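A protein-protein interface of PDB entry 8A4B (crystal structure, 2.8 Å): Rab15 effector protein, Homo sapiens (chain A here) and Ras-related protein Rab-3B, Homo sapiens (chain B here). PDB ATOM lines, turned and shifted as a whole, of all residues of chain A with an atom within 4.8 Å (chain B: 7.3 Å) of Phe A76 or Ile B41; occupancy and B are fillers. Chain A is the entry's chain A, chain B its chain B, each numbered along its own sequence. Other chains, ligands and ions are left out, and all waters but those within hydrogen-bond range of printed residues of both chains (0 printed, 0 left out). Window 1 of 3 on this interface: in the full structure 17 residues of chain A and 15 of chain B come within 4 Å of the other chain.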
ATOM      1  N   MET A  68     -27.182  13.692  12.434  1.00  0.00           N
ATOM      2  CA  MET A  68     -26.614  12.372  12.218  1.00  0.00           C
ATOM      3  C   MET A  68     -26.338  11.700  13.552  1.00  0.00           C
ATOM      4  O   MET A  68     -25.902  12.342  14.510  1.00  0.00           O
ATOM      5  CB  MET A  68     -25.322  12.467  11.406  1.00  0.00           C
ATOM      6  CG  MET A  68     -25.472  13.176  10.066  1.00  0.00           C
ATOM      7  SD  MET A  68     -26.557  12.324   8.899  1.00  0.00           S
ATOM      8  CE  MET A  68     -28.102  13.193   9.138  1.00  0.00           C
ATOM      9  N   GLN A  72     -23.767   7.563  11.793  1.00  0.00           N
ATOM     10  CA  GLN A  72     -23.953   8.363  10.587  1.00  0.00           C
ATOM     11  C   GLN A  72     -22.917   9.477  10.491  1.00  0.00           C
ATOM     12  O   GLN A  72     -22.394   9.748   9.407  1.00  0.00           O
ATOM     13  CB  GLN A  72     -25.369   8.933  10.545  1.00  0.00           C
ATOM     14  CG  GLN A  72     -26.395   7.961   9.993  1.00  0.00           C
ATOM     15  CD  GLN A  72     -27.804   8.493  10.087  1.00  0.00           C
ATOM     16  OE1 GLN A  72     -28.139   9.243  11.008  1.00  0.00           O
ATOM     17  NE2 GLN A  72     -28.643   8.112   9.133  1.00  0.00           N
ATOM     18  N   ALA A  73     -22.605  10.133  11.610  1.00  0.00           N
ATOM     19  CA  ALA A  73     -21.579  11.167  11.581  1.00  0.00           C
ATOM     20  C   ALA A  73     -20.235  10.595  11.154  1.00  0.00           C
ATOM     21  O   ALA A  73     -19.515  11.208  10.358  1.00  0.00           O
ATOM     22  CB  ALA A  73     -21.466  11.839  12.951  1.00  0.00           C
ATOM     23  N   PHE A  74     -19.877   9.420  11.673  1.00  0.00           N
ATOM     24  CA  PHE A  74     -18.612   8.808  11.281  1.00  0.00           C
ATOM     25  C   PHE A  74     -18.610   8.422   9.807  1.00  0.00           C
ATOM     26  O   PHE A  74     -17.618   8.644   9.105  1.00  0.00           O
ATOM     27  CB  PHE A  74     -18.328   7.590  12.152  1.00  0.00           C
ATOM     28  CG  PHE A  74     -17.132   6.802  11.712  1.00  0.00           C
ATOM     29  CD1 PHE A  74     -15.852   7.229  12.021  1.00  0.00           C
ATOM     30  CD2 PHE A  74     -17.286   5.631  10.991  1.00  0.00           C
ATOM     31  CE1 PHE A  74     -14.750   6.505  11.617  1.00  0.00           C
ATOM     32  CE2 PHE A  74     -16.187   4.901  10.587  1.00  0.00           C
ATOM     33  CZ  PHE A  74     -14.917   5.339  10.901  1.00  0.00           C
ATOM     34  N   LEU A  75     -19.709   7.837   9.320  1.00  0.00           N
ATOM     35  CA  LEU A  75     -19.727   7.327   7.951  1.00  0.00           C
ATOM     36  C   LEU A  75     -19.797   8.450   6.925  1.00  0.00           C
ATOM     37  O   LEU A  75     -19.090   8.416   5.912  1.00  0.00           O
ATOM     38  CB  LEU A  75     -20.908   6.379   7.760  1.00  0.00           C
ATOM     39  CG  LEU A  75     -20.838   5.017   8.440  1.00  0.00           C
ATOM     40  CD1 LEU A  75     -22.165   4.302   8.278  1.00  0.00           C
ATOM     41  CD2 LEU A  75     -19.707   4.186   7.860  1.00  0.00           C
ATOM     42  N   PHE A  76     -20.650   9.444   7.159  1.00  0.00           N
ATOM     43  CA  PHE A  76     -20.980  10.434   6.148  1.00  0.00           C
ATOM     44  C   PHE A  76     -20.083  11.655   6.176  1.00  0.00           C
ATOM     45  O   PHE A  76     -20.197  12.500   5.283  1.00  0.00           O
ATOM     46  CB  PHE A  76     -22.426  10.907   6.312  1.00  0.00           C
ATOM     47  CG  PHE A  76     -23.442   9.816   6.198  1.00  0.00           C
ATOM     48  CD1 PHE A  76     -23.135   8.619   5.564  1.00  0.00           C
ATOM     49  CD2 PHE A  76     -24.714   9.993   6.717  1.00  0.00           C
ATOM     50  CE1 PHE A  76     -24.074   7.617   5.463  1.00  0.00           C
ATOM     51  CE2 PHE A  76     -25.660   8.997   6.618  1.00  0.00           C
ATOM     52  CZ  PHE A  76     -25.342   7.803   5.992  1.00  0.00           C
ATOM     53  N   GLY A  77     -19.211  11.786   7.169  1.00  0.00           N
ATOM     54  CA  GLY A  77     -18.473  13.027   7.312  1.00  0.00           C
ATOM     55  C   GLY A  77     -19.370  14.234   7.465  1.00  0.00           C
ATOM     56  O   GLY A  77     -18.980  15.345   7.097  1.00  0.00           O
ATOM     57  N   ALA A  78     -20.573  14.041   7.991  1.00  0.00           N
ATOM     58  CA  ALA A  78     -21.528  15.114   8.199  1.00  0.00           C
ATOM     59  C   ALA A  78     -22.006  15.082   9.643  1.00  0.00           C
ATOM     60  O   ALA A  78     -22.151  14.013  10.242  1.00  0.00           O
ATOM     61  CB  ALA A  78     -22.726  14.990   7.248  1.00  0.00           C
ATOM     62  N   LYS A 134     -14.732  11.800   3.385  1.00  0.00           N
ATOM     63  CA  LYS A 134     -16.014  11.156   3.627  1.00  0.00           C
ATOM     64  C   LYS A 134     -17.169  12.081   3.261  1.00  0.00           C
ATOM     65  O   LYS A 134     -18.156  11.638   2.665  1.00  0.00           O
ATOM     66  CB  LYS A 134     -16.103  10.692   5.082  1.00  0.00           C
ATOM     67  CG  LYS A 134     -15.217   9.479   5.376  1.00  0.00           C
ATOM     68  CD  LYS A 134     -15.412   8.918   6.785  1.00  0.00           C
ATOM     69  CE  LYS A 134     -14.807   9.827   7.849  1.00  0.00           C
ATOM     70  NZ  LYS A 134     -14.762   9.186   9.190  1.00  0.00           N
ATOM     71  N   LEU A 135     -17.057  13.373   3.584  1.00  0.00           N
ATOM     72  CA  LEU A 135     -18.111  14.313   3.212  1.00  0.00           C
ATOM     73  C   LEU A 135     -18.197  14.481   1.697  1.00  0.00           C
ATOM     74  O   LEU A 135     -19.298  14.545   1.131  1.00  0.00           O
ATOM     75  CB  LEU A 135     -17.881  15.666   3.888  1.00  0.00           C
ATOM     76  CG  LEU A 135     -18.914  16.753   3.573  1.00  0.00           C
ATOM     77  CD1 LEU A 135     -20.321  16.263   3.884  1.00  0.00           C
ATOM     78  CD2 LEU A 135     -18.613  18.036   4.333  1.00  0.00           C
ATOM     79  N   PHE A 138     -19.842  11.395   0.339  1.00  0.00           N
ATOM     80  CA  PHE A 138     -21.262  11.408   0.664  1.00  0.00           C
ATOM     81  C   PHE A 138     -22.026  12.319  -0.289  1.00  0.00           C
ATOM     82  O   PHE A 138     -23.062  11.932  -0.843  1.00  0.00           O
ATOM     83  CB  PHE A 138     -21.460  11.852   2.114  1.00  0.00           C
ATOM     84  CG  PHE A 138     -22.895  11.909   2.534  1.00  0.00           C
ATOM     85  CD1 PHE A 138     -23.586  10.747   2.829  1.00  0.00           C
ATOM     86  CD2 PHE A 138     -23.555  13.120   2.627  1.00  0.00           C
ATOM     87  CE1 PHE A 138     -24.907  10.791   3.207  1.00  0.00           C
ATOM     88  CE2 PHE A 138     -24.878  13.172   3.008  1.00  0.00           C
ATOM     89  CZ  PHE A 138     -25.555  12.006   3.297  1.00  0.00           C
ATOM     90  N   LYS B   8     -22.271  -9.398   7.700  1.00  0.00           N
ATOM     91  CA  LYS B   8     -22.871  -8.146   7.267  1.00  0.00           C
ATOM     92  C   LYS B   8     -24.244  -8.434   6.669  1.00  0.00           C
ATOM     93  O   LYS B   8     -24.375  -9.209   5.703  1.00  0.00           O
ATOM     94  CB  LYS B   8     -21.983  -7.418   6.259  1.00  0.00           C
ATOM     95  CG  LYS B   8     -22.485  -6.015   5.927  1.00  0.00           C
ATOM     96  CD  LYS B   8     -21.591  -5.297   4.939  1.00  0.00           C
ATOM     97  CE  LYS B   8     -22.067  -3.871   4.717  1.00  0.00           C
ATOM     98  NZ  LYS B   8     -21.207  -3.139   3.742  1.00  0.00           N
ATOM     99  N   LEU B  10     -27.923  -6.530   5.333  1.00  0.00           N
ATOM    100  CA  LEU B  10     -28.548  -5.290   4.906  1.00  0.00           C
ATOM    101  C   LEU B  10     -30.051  -5.487   4.845  1.00  0.00           C
ATOM    102  O   LEU B  10     -30.533  -6.594   4.598  1.00  0.00           O
ATOM    103  CB  LEU B  10     -28.030  -4.815   3.548  1.00  0.00           C
ATOM    104  CG  LEU B  10     -26.850  -3.848   3.633  1.00  0.00           C
ATOM    105  CD1 LEU B  10     -25.582  -4.602   3.965  1.00  0.00           C
ATOM    106  CD2 LEU B  10     -26.698  -3.057   2.352  1.00  0.00           C
ATOM    107  N   ILE B  11     -30.781  -4.409   5.114  1.00  0.00           N
ATOM    108  CA  ILE B  11     -32.236  -4.402   5.067  1.00  0.00           C
ATOM    109  C   ILE B  11     -32.648  -3.368   4.037  1.00  0.00           C
ATOM    110  O   ILE B  11     -32.350  -2.171   4.197  1.00  0.00           O
ATOM    111  CB  ILE B  11     -32.855  -4.085   6.434  1.00  0.00           C
ATOM    112  CG1 ILE B  11     -32.293  -5.014   7.508  1.00  0.00           C
ATOM    113  CG2 ILE B  11     -34.361  -4.232   6.371  1.00  0.00           C
ATOM    114  CD1 ILE B  11     -32.931  -4.798   8.851  1.00  0.00           C
ATOM    115  N   THR B  38     -35.196   7.124   7.324  1.00  0.00           N
ATOM    116  CA  THR B  38     -33.747   7.015   7.428  1.00  0.00           C
ATOM    117  C   THR B  38     -33.068   7.869   6.365  1.00  0.00           C
ATOM    118  O   THR B  38     -33.472   7.863   5.198  1.00  0.00           O
ATOM    119  CB  THR B  38     -33.313   5.553   7.300  1.00  0.00           C
ATOM    120  OG1 THR B  38     -33.718   4.829   8.475  1.00  0.00           O
ATOM    121  CG2 THR B  38     -31.795   5.440   7.136  1.00  0.00           C
ATOM    122  N   VAL B  39     -32.046   8.613   6.771  1.00  0.00           N
ATOM    123  CA  VAL B  39     -31.308   9.490   5.871  1.00  0.00           C
ATOM    124  C   VAL B  39     -30.079   8.722   5.399  1.00  0.00           C
ATOM    125  O   VAL B  39     -29.080   8.609   6.114  1.00  0.00           O
ATOM    126  CB  VAL B  39     -30.935  10.812   6.542  1.00  0.00           C
ATOM    127  CG1 VAL B  39     -30.024  11.617   5.640  1.00  0.00           C
ATOM    128  CG2 VAL B  39     -32.198  11.596   6.870  1.00  0.00           C
ATOM    129  N   GLY B  40     -30.155   8.186   4.189  1.00  0.00           N
ATOM    130  CA  GLY B  40     -29.043   7.474   3.599  1.00  0.00           C
ATOM    131  C   GLY B  40     -28.930   6.052   4.104  1.00  0.00           C
ATOM    132  O   GLY B  40     -29.384   5.123   3.438  1.00  0.00           O
ATOM    133  N   ILE B  41     -28.350   5.865   5.289  1.00  0.00           N
ATOM    134  CA  ILE B  41     -28.153   4.531   5.837  1.00  0.00           C
ATOM    135  C   ILE B  41     -27.772   4.668   7.301  1.00  0.00           C
ATOM    136  O   ILE B  41     -27.289   5.722   7.730  1.00  0.00           O
ATOM    137  CB  ILE B  41     -27.070   3.770   5.022  1.00  0.00           C
ATOM    138  CG1 ILE B  41     -27.195   2.262   5.238  1.00  0.00           C
ATOM    139  CG2 ILE B  41     -25.673   4.275   5.375  1.00  0.00           C
ATOM    140  CD1 ILE B  41     -26.400   1.439   4.246  1.00  0.00           C
ATOM    141  N   ASP B  42     -28.021   3.617   8.079  1.00  0.00           N
ATOM    142  CA  ASP B  42     -27.505   3.536   9.444  1.00  0.00           C
ATOM    143  C   ASP B  42     -27.237   2.068   9.753  1.00  0.00           C
ATOM    144  O   ASP B  42     -27.483   1.197   8.917  1.00  0.00           O
ATOM    145  CB  ASP B  42     -28.471   4.177  10.444  1.00  0.00           C
ATOM    146  CG  ASP B  42     -27.754   4.776  11.637  1.00  0.00           C
ATOM    147  OD1 ASP B  42     -26.723   4.207  12.059  1.00  0.00           O
ATOM    148  OD2 ASP B  42     -28.215   5.818  12.148  1.00  0.00           O
ATOM    149  N   PHE B  43     -26.712   1.779  10.944  1.00  0.00           N
ATOM    150  CA  PHE B  43     -26.464   0.375  11.266  1.00  0.00           C
ATOM    151  C   PHE B  43     -26.424   0.145  12.774  1.00  0.00           C
ATOM    152  O   PHE B  43     -26.162   1.056  13.566  1.00  0.00           O
ATOM    153  CB  PHE B  43     -25.173  -0.136  10.607  1.00  0.00           C
ATOM    154  CG  PHE B  43     -23.907   0.318  11.288  1.00  0.00           C
ATOM    155  CD1 PHE B  43     -23.299   1.506  10.924  1.00  0.00           C
ATOM    156  CD2 PHE B  43     -23.310  -0.465  12.266  1.00  0.00           C
ATOM    157  CE1 PHE B  43     -22.129   1.916  11.536  1.00  0.00           C
ATOM    158  CE2 PHE B  43     -22.143  -0.058  12.882  1.00  0.00           C
ATOM    159  CZ  PHE B  43     -21.552   1.133  12.518  1.00  0.00           C
ATOM    160  N   TRP B  60     -27.334  -3.318   8.627  1.00  0.00           N
ATOM    161  CA  TRP B  60     -27.452  -2.000   8.031  1.00  0.00           C
ATOM    162  C   TRP B  60     -28.897  -1.776   7.627  1.00  0.00           C
ATOM    163  O   TRP B  60     -29.521  -2.650   7.022  1.00  0.00           O
ATOM    164  CB  TRP B  60     -26.514  -1.855   6.831  1.00  0.00           C
ATOM    165  CG  TRP B  60     -25.066  -1.982   7.209  1.00  0.00           C
ATOM    166  CD1 TRP B  60     -24.421  -3.117   7.607  1.00  0.00           C
ATOM    167  CD2 TRP B  60     -24.085  -0.940   7.226  1.00  0.00           C
ATOM    168  NE1 TRP B  60     -23.102  -2.848   7.872  1.00  0.00           N
ATOM    169  CE2 TRP B  60     -22.869  -1.518   7.648  1.00  0.00           C
ATOM    170  CE3 TRP B  60     -24.115   0.423   6.925  1.00  0.00           C
ATOM    171  CZ2 TRP B  60     -21.697  -0.779   7.776  1.00  0.00           C
ATOM    172  CZ3 TRP B  60     -22.948   1.155   7.052  1.00  0.00           C
ATOM    173  CH2 TRP B  60     -21.756   0.552   7.475  1.00  0.00           C
ATOM    174  N   ASP B  61     -29.436  -0.641   8.037  1.00  0.00           N
ATOM    175  CA  ASP B  61     -30.769  -0.191   7.672  1.00  0.00           C
ATOM    176  C   ASP B  61     -30.611   0.793   6.520  1.00  0.00           C
ATOM    177  O   ASP B  61     -30.073   1.893   6.714  1.00  0.00           O
ATOM    178  CB  ASP B  61     -31.427   0.447   8.894  1.00  0.00           C
ATOM    179  CG  ASP B  61     -32.796   1.035   8.609  1.00  0.00           C
ATOM    180  OD1 ASP B  61     -33.306   0.936   7.472  1.00  0.00           O
ATOM    181  OD2 ASP B  61     -33.369   1.610   9.556  1.00  0.00           O
ATOM    182  N   THR B  62     -31.051   0.400   5.319  1.00  0.00           N
ATOM    183  CA  THR B  62     -30.915   1.295   4.180  1.00  0.00           C
ATOM    184  C   THR B  62     -32.155   2.176   4.045  1.00  0.00           C
ATOM    185  O   THR B  62     -33.213   1.892   4.607  1.00  0.00           O
ATOM    186  CB  THR B  62     -30.685   0.494   2.900  1.00  0.00           C
ATOM    187  OG1 THR B  62     -31.743  -0.457   2.743  1.00  0.00           O
ATOM    188  CG2 THR B  62     -29.357  -0.252   2.977  1.00  0.00           C
ATOM    189  N   ALA B  63     -32.004   3.270   3.310  1.00  0.00           N
ATOM    190  CA  ALA B  63     -33.130   4.145   3.019  1.00  0.00           C
ATOM    191  C   ALA B  63     -33.872   3.639   1.789  1.00  0.00           C
ATOM    192  O   ALA B  63     -33.269   3.091   0.864  1.00  0.00           O
ATOM    193  CB  ALA B  63     -32.662   5.586   2.803  1.00  0.00           C
ATOM    194  N   TYR B  68     -31.740   8.108  -2.259  1.00  0.00           N
ATOM    195  CA  TYR B  68     -30.580   7.489  -1.633  1.00  0.00           C
ATOM    196  C   TYR B  68     -30.175   6.179  -2.296  1.00  0.00           C
ATOM    197  O   TYR B  68     -29.192   5.558  -1.869  1.00  0.00           O
ATOM    198  CB  TYR B  68     -30.845   7.259  -0.139  1.00  0.00           C
ATOM    199  CG  TYR B  68     -31.285   8.510   0.587  1.00  0.00           C
ATOM    200  CD1 TYR B  68     -30.437   9.603   0.698  1.00  0.00           C
ATOM    201  CD2 TYR B  68     -32.552   8.601   1.151  1.00  0.00           C
ATOM    202  CE1 TYR B  68     -30.837  10.751   1.353  1.00  0.00           C
ATOM    203  CE2 TYR B  68     -32.958   9.741   1.810  1.00  0.00           C
ATOM    204  CZ  TYR B  68     -32.096  10.815   1.909  1.00  0.00           C
ATOM    205  OH  TYR B  68     -32.497  11.956   2.564  1.00  0.00           O
ATOM    206  N   ILE B  71     -26.416   6.037  -2.897  1.00  0.00           N
ATOM    207  CA  ILE B  71     -25.522   5.922  -1.743  1.00  0.00           C
ATOM    208  C   ILE B  71     -25.703   4.566  -1.069  1.00  0.00           C
ATOM    209  O   ILE B  71     -24.726   3.860  -0.780  1.00  0.00           O
ATOM    210  CB  ILE B  71     -25.726   7.094  -0.761  1.00  0.00           C
ATOM    211  CG1 ILE B  71     -24.965   6.852   0.543  1.00  0.00           C
ATOM    212  CG2 ILE B  71     -27.183   7.335  -0.460  1.00  0.00           C
ATOM    213  CD1 ILE B  71     -23.478   6.883   0.405  1.00  0.00           C
ATOM    214  N   THR B  72     -26.960   4.150  -0.875  1.00  0.00           N
ATOM    215  CA  THR B  72     -27.218   2.841  -0.283  1.00  0.00           C
ATOM    216  C   THR B  72     -26.520   1.738  -1.063  1.00  0.00           C
ATOM    217  O   THR B  72     -25.937   0.826  -0.466  1.00  0.00           O
ATOM    218  CB  THR B  72     -28.720   2.558  -0.217  1.00  0.00           C
ATOM    219  OG1 THR B  72     -29.304   2.747  -1.512  1.00  0.00           O
ATOM    220  CG2 THR B  72     -29.396   3.470   0.781  1.00  0.00           C
ATOM    221  N   THR B  73     -26.544   1.813  -2.399  1.00  0.00           N
ATOM    222  CA  THR B  73     -25.952   0.731  -3.176  1.00  0.00           C
ATOM    223  C   THR B  73     -24.468   0.595  -2.885  1.00  0.00           C
ATOM    224  O   THR B  73     -23.946  -0.526  -2.850  1.00  0.00           O
ATOM    225  CB  THR B  73     -26.185   0.930  -4.678  1.00  0.00           C
ATOM    226  OG1 THR B  73     -26.114   2.323  -5.011  1.00  0.00           O
ATOM    227  CG2 THR B  73     -27.537   0.361  -5.093  1.00  0.00           C
ATOM    228  N   ALA B  74     -23.780   1.714  -2.632  1.00  0.00           N
ATOM    229  CA  ALA B  74     -22.353   1.630  -2.347  1.00  0.00           C
ATOM    230  C   ALA B  74     -22.087   0.766  -1.122  1.00  0.00           C
ATOM    231  O   ALA B  74     -21.039   0.116  -1.036  1.00  0.00           O
ATOM    232  CB  ALA B  74     -21.768   3.028  -2.156  1.00  0.00           C
ATOM    233  N   TYR B  75     -23.029   0.719  -0.182  1.00  0.00           N
ATOM    234  CA  TYR B  75     -22.857  -0.051   1.039  1.00  0.00           C
ATOM    235  C   TYR B  75     -23.278  -1.505   0.897  1.00  0.00           C
ATOM    236  O   TYR B  75     -23.174  -2.259   1.871  1.00  0.00           O
ATOM    237  CB  TYR B  75     -23.626   0.600   2.187  1.00  0.00           C
ATOM    238  CG  TYR B  75     -22.974   1.866   2.679  1.00  0.00           C
ATOM    239  CD1 TYR B  75     -21.976   1.825   3.640  1.00  0.00           C
ATOM    240  CD2 TYR B  75     -23.345   3.103   2.172  1.00  0.00           C
ATOM    241  CE1 TYR B  75     -21.374   2.983   4.090  1.00  0.00           C
ATOM    242  CE2 TYR B  75     -22.751   4.264   2.618  1.00  0.00           C
ATOM    243  CZ  TYR B  75     -21.766   4.199   3.574  1.00  0.00           C
ATOM    244  OH  TYR B  75     -21.169   5.357   4.019  1.00  0.00           O
ATOM    245  N   TYR B  76     -23.748  -1.923  -0.281  1.00  0.00           N
ATOM    246  CA  TYR B  76     -23.955  -3.348  -0.507  1.00  0.00           C
ATOM    247  C   TYR B  76     -22.636  -4.111  -0.533  1.00  0.00           C
ATOM    248  O   TYR B  76     -22.647  -5.342  -0.426  1.00  0.00           O
ATOM    249  CB  TYR B  76     -24.705  -3.597  -1.820  1.00  0.00           C
ATOM    250  CG  TYR B  76     -26.170  -3.189  -1.861  1.00  0.00           C
ATOM    251  CD1 TYR B  76     -26.640  -2.097  -1.148  1.00  0.00           C
ATOM    252  CD2 TYR B  76     -27.081  -3.902  -2.636  1.00  0.00           C
ATOM    253  CE1 TYR B  76     -27.975  -1.725  -1.202  1.00  0.00           C
ATOM    254  CE2 TYR B  76     -28.415  -3.538  -2.696  1.00  0.00           C
ATOM    255  CZ  TYR B  76     -28.857  -2.449  -1.976  1.00  0.00           C
ATOM    256  OH  TYR B  76     -30.186  -2.081  -2.029  1.00  0.00           O
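Among the printed residues, pairs that only touch across the chains: Phe A76 with Ile B41 (3.3 Å), Gln A72 with Asp B42 (3.4 Å), Leu A75 with Trp B60 (3.5 Å), Phe A76 with Val B39 (3.5 Å), Leu A75 with Tyr B75 (3.9 Å) and Phe A76 with Tyr B75 (3.95 Å).
Of chain B, only Val B39 (3.5 Å), Ile B41 (3.3 Å) and Tyr B75 (3.95 Å) come within 4 Å of Phe A76. Of chain A, only Gln A72 and Phe A76 come within 4 Å of Ile B41. Of the printed residues of chain A, Val B39 touches Gln A72 and Phe A76. Of the printed residues of chain B, Leu A75 touches Trp B60 and Tyr B75. Printed residues of chain A within 4 Å of Trp B60: Leu A75. Of the printed residues of chain A, Asp B42 touches Gln A72. Of the printed residues of chain B, Gln A72 touches Val B39, Ile B41 and Asp B42. Ala A73 touches none of the printed residues of chain B. Ala A78 touches none of the printed residues of chain B. The nearest residue of chain A that does not touch Ile B41 is Leu A75 (4.6 Å).
The side-chain amide nitrogen (NE2) of Gln A72 lies within hydrogen-bond range of the backbone carbonyl oxygen (O) of Val B39, at 3.1 Å. The side-chain amide nitrogen (NE2) of Gln A72 sits at hydrogen-bond distance from the backbone carbonyl oxygen (O) of Ile B41, 3.1 Å away.
NZ of Lys B8 lies within hydrogen-bond range of O of Tyr B75 (2.9 Å). The backbone NH (N) of Ile B11 is in hydrogen-bond range of the backbone carbonyl oxygen (O) of Trp B60, 2.9 Å away. O of Asp B42 lies within hydrogen-bond range of N of Asp B61, 2.8 Å away.
Of the 20 printed residues of chain B, 5 touch a printed residue of chain A. Hydrophobic or aromatic side chains of chain B that line the printed part of chain A: Ile B41, Trp B60 and Tyr B75. Along chain B the printed residues that touch a printed residue of chain A span positions 39 to 75.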
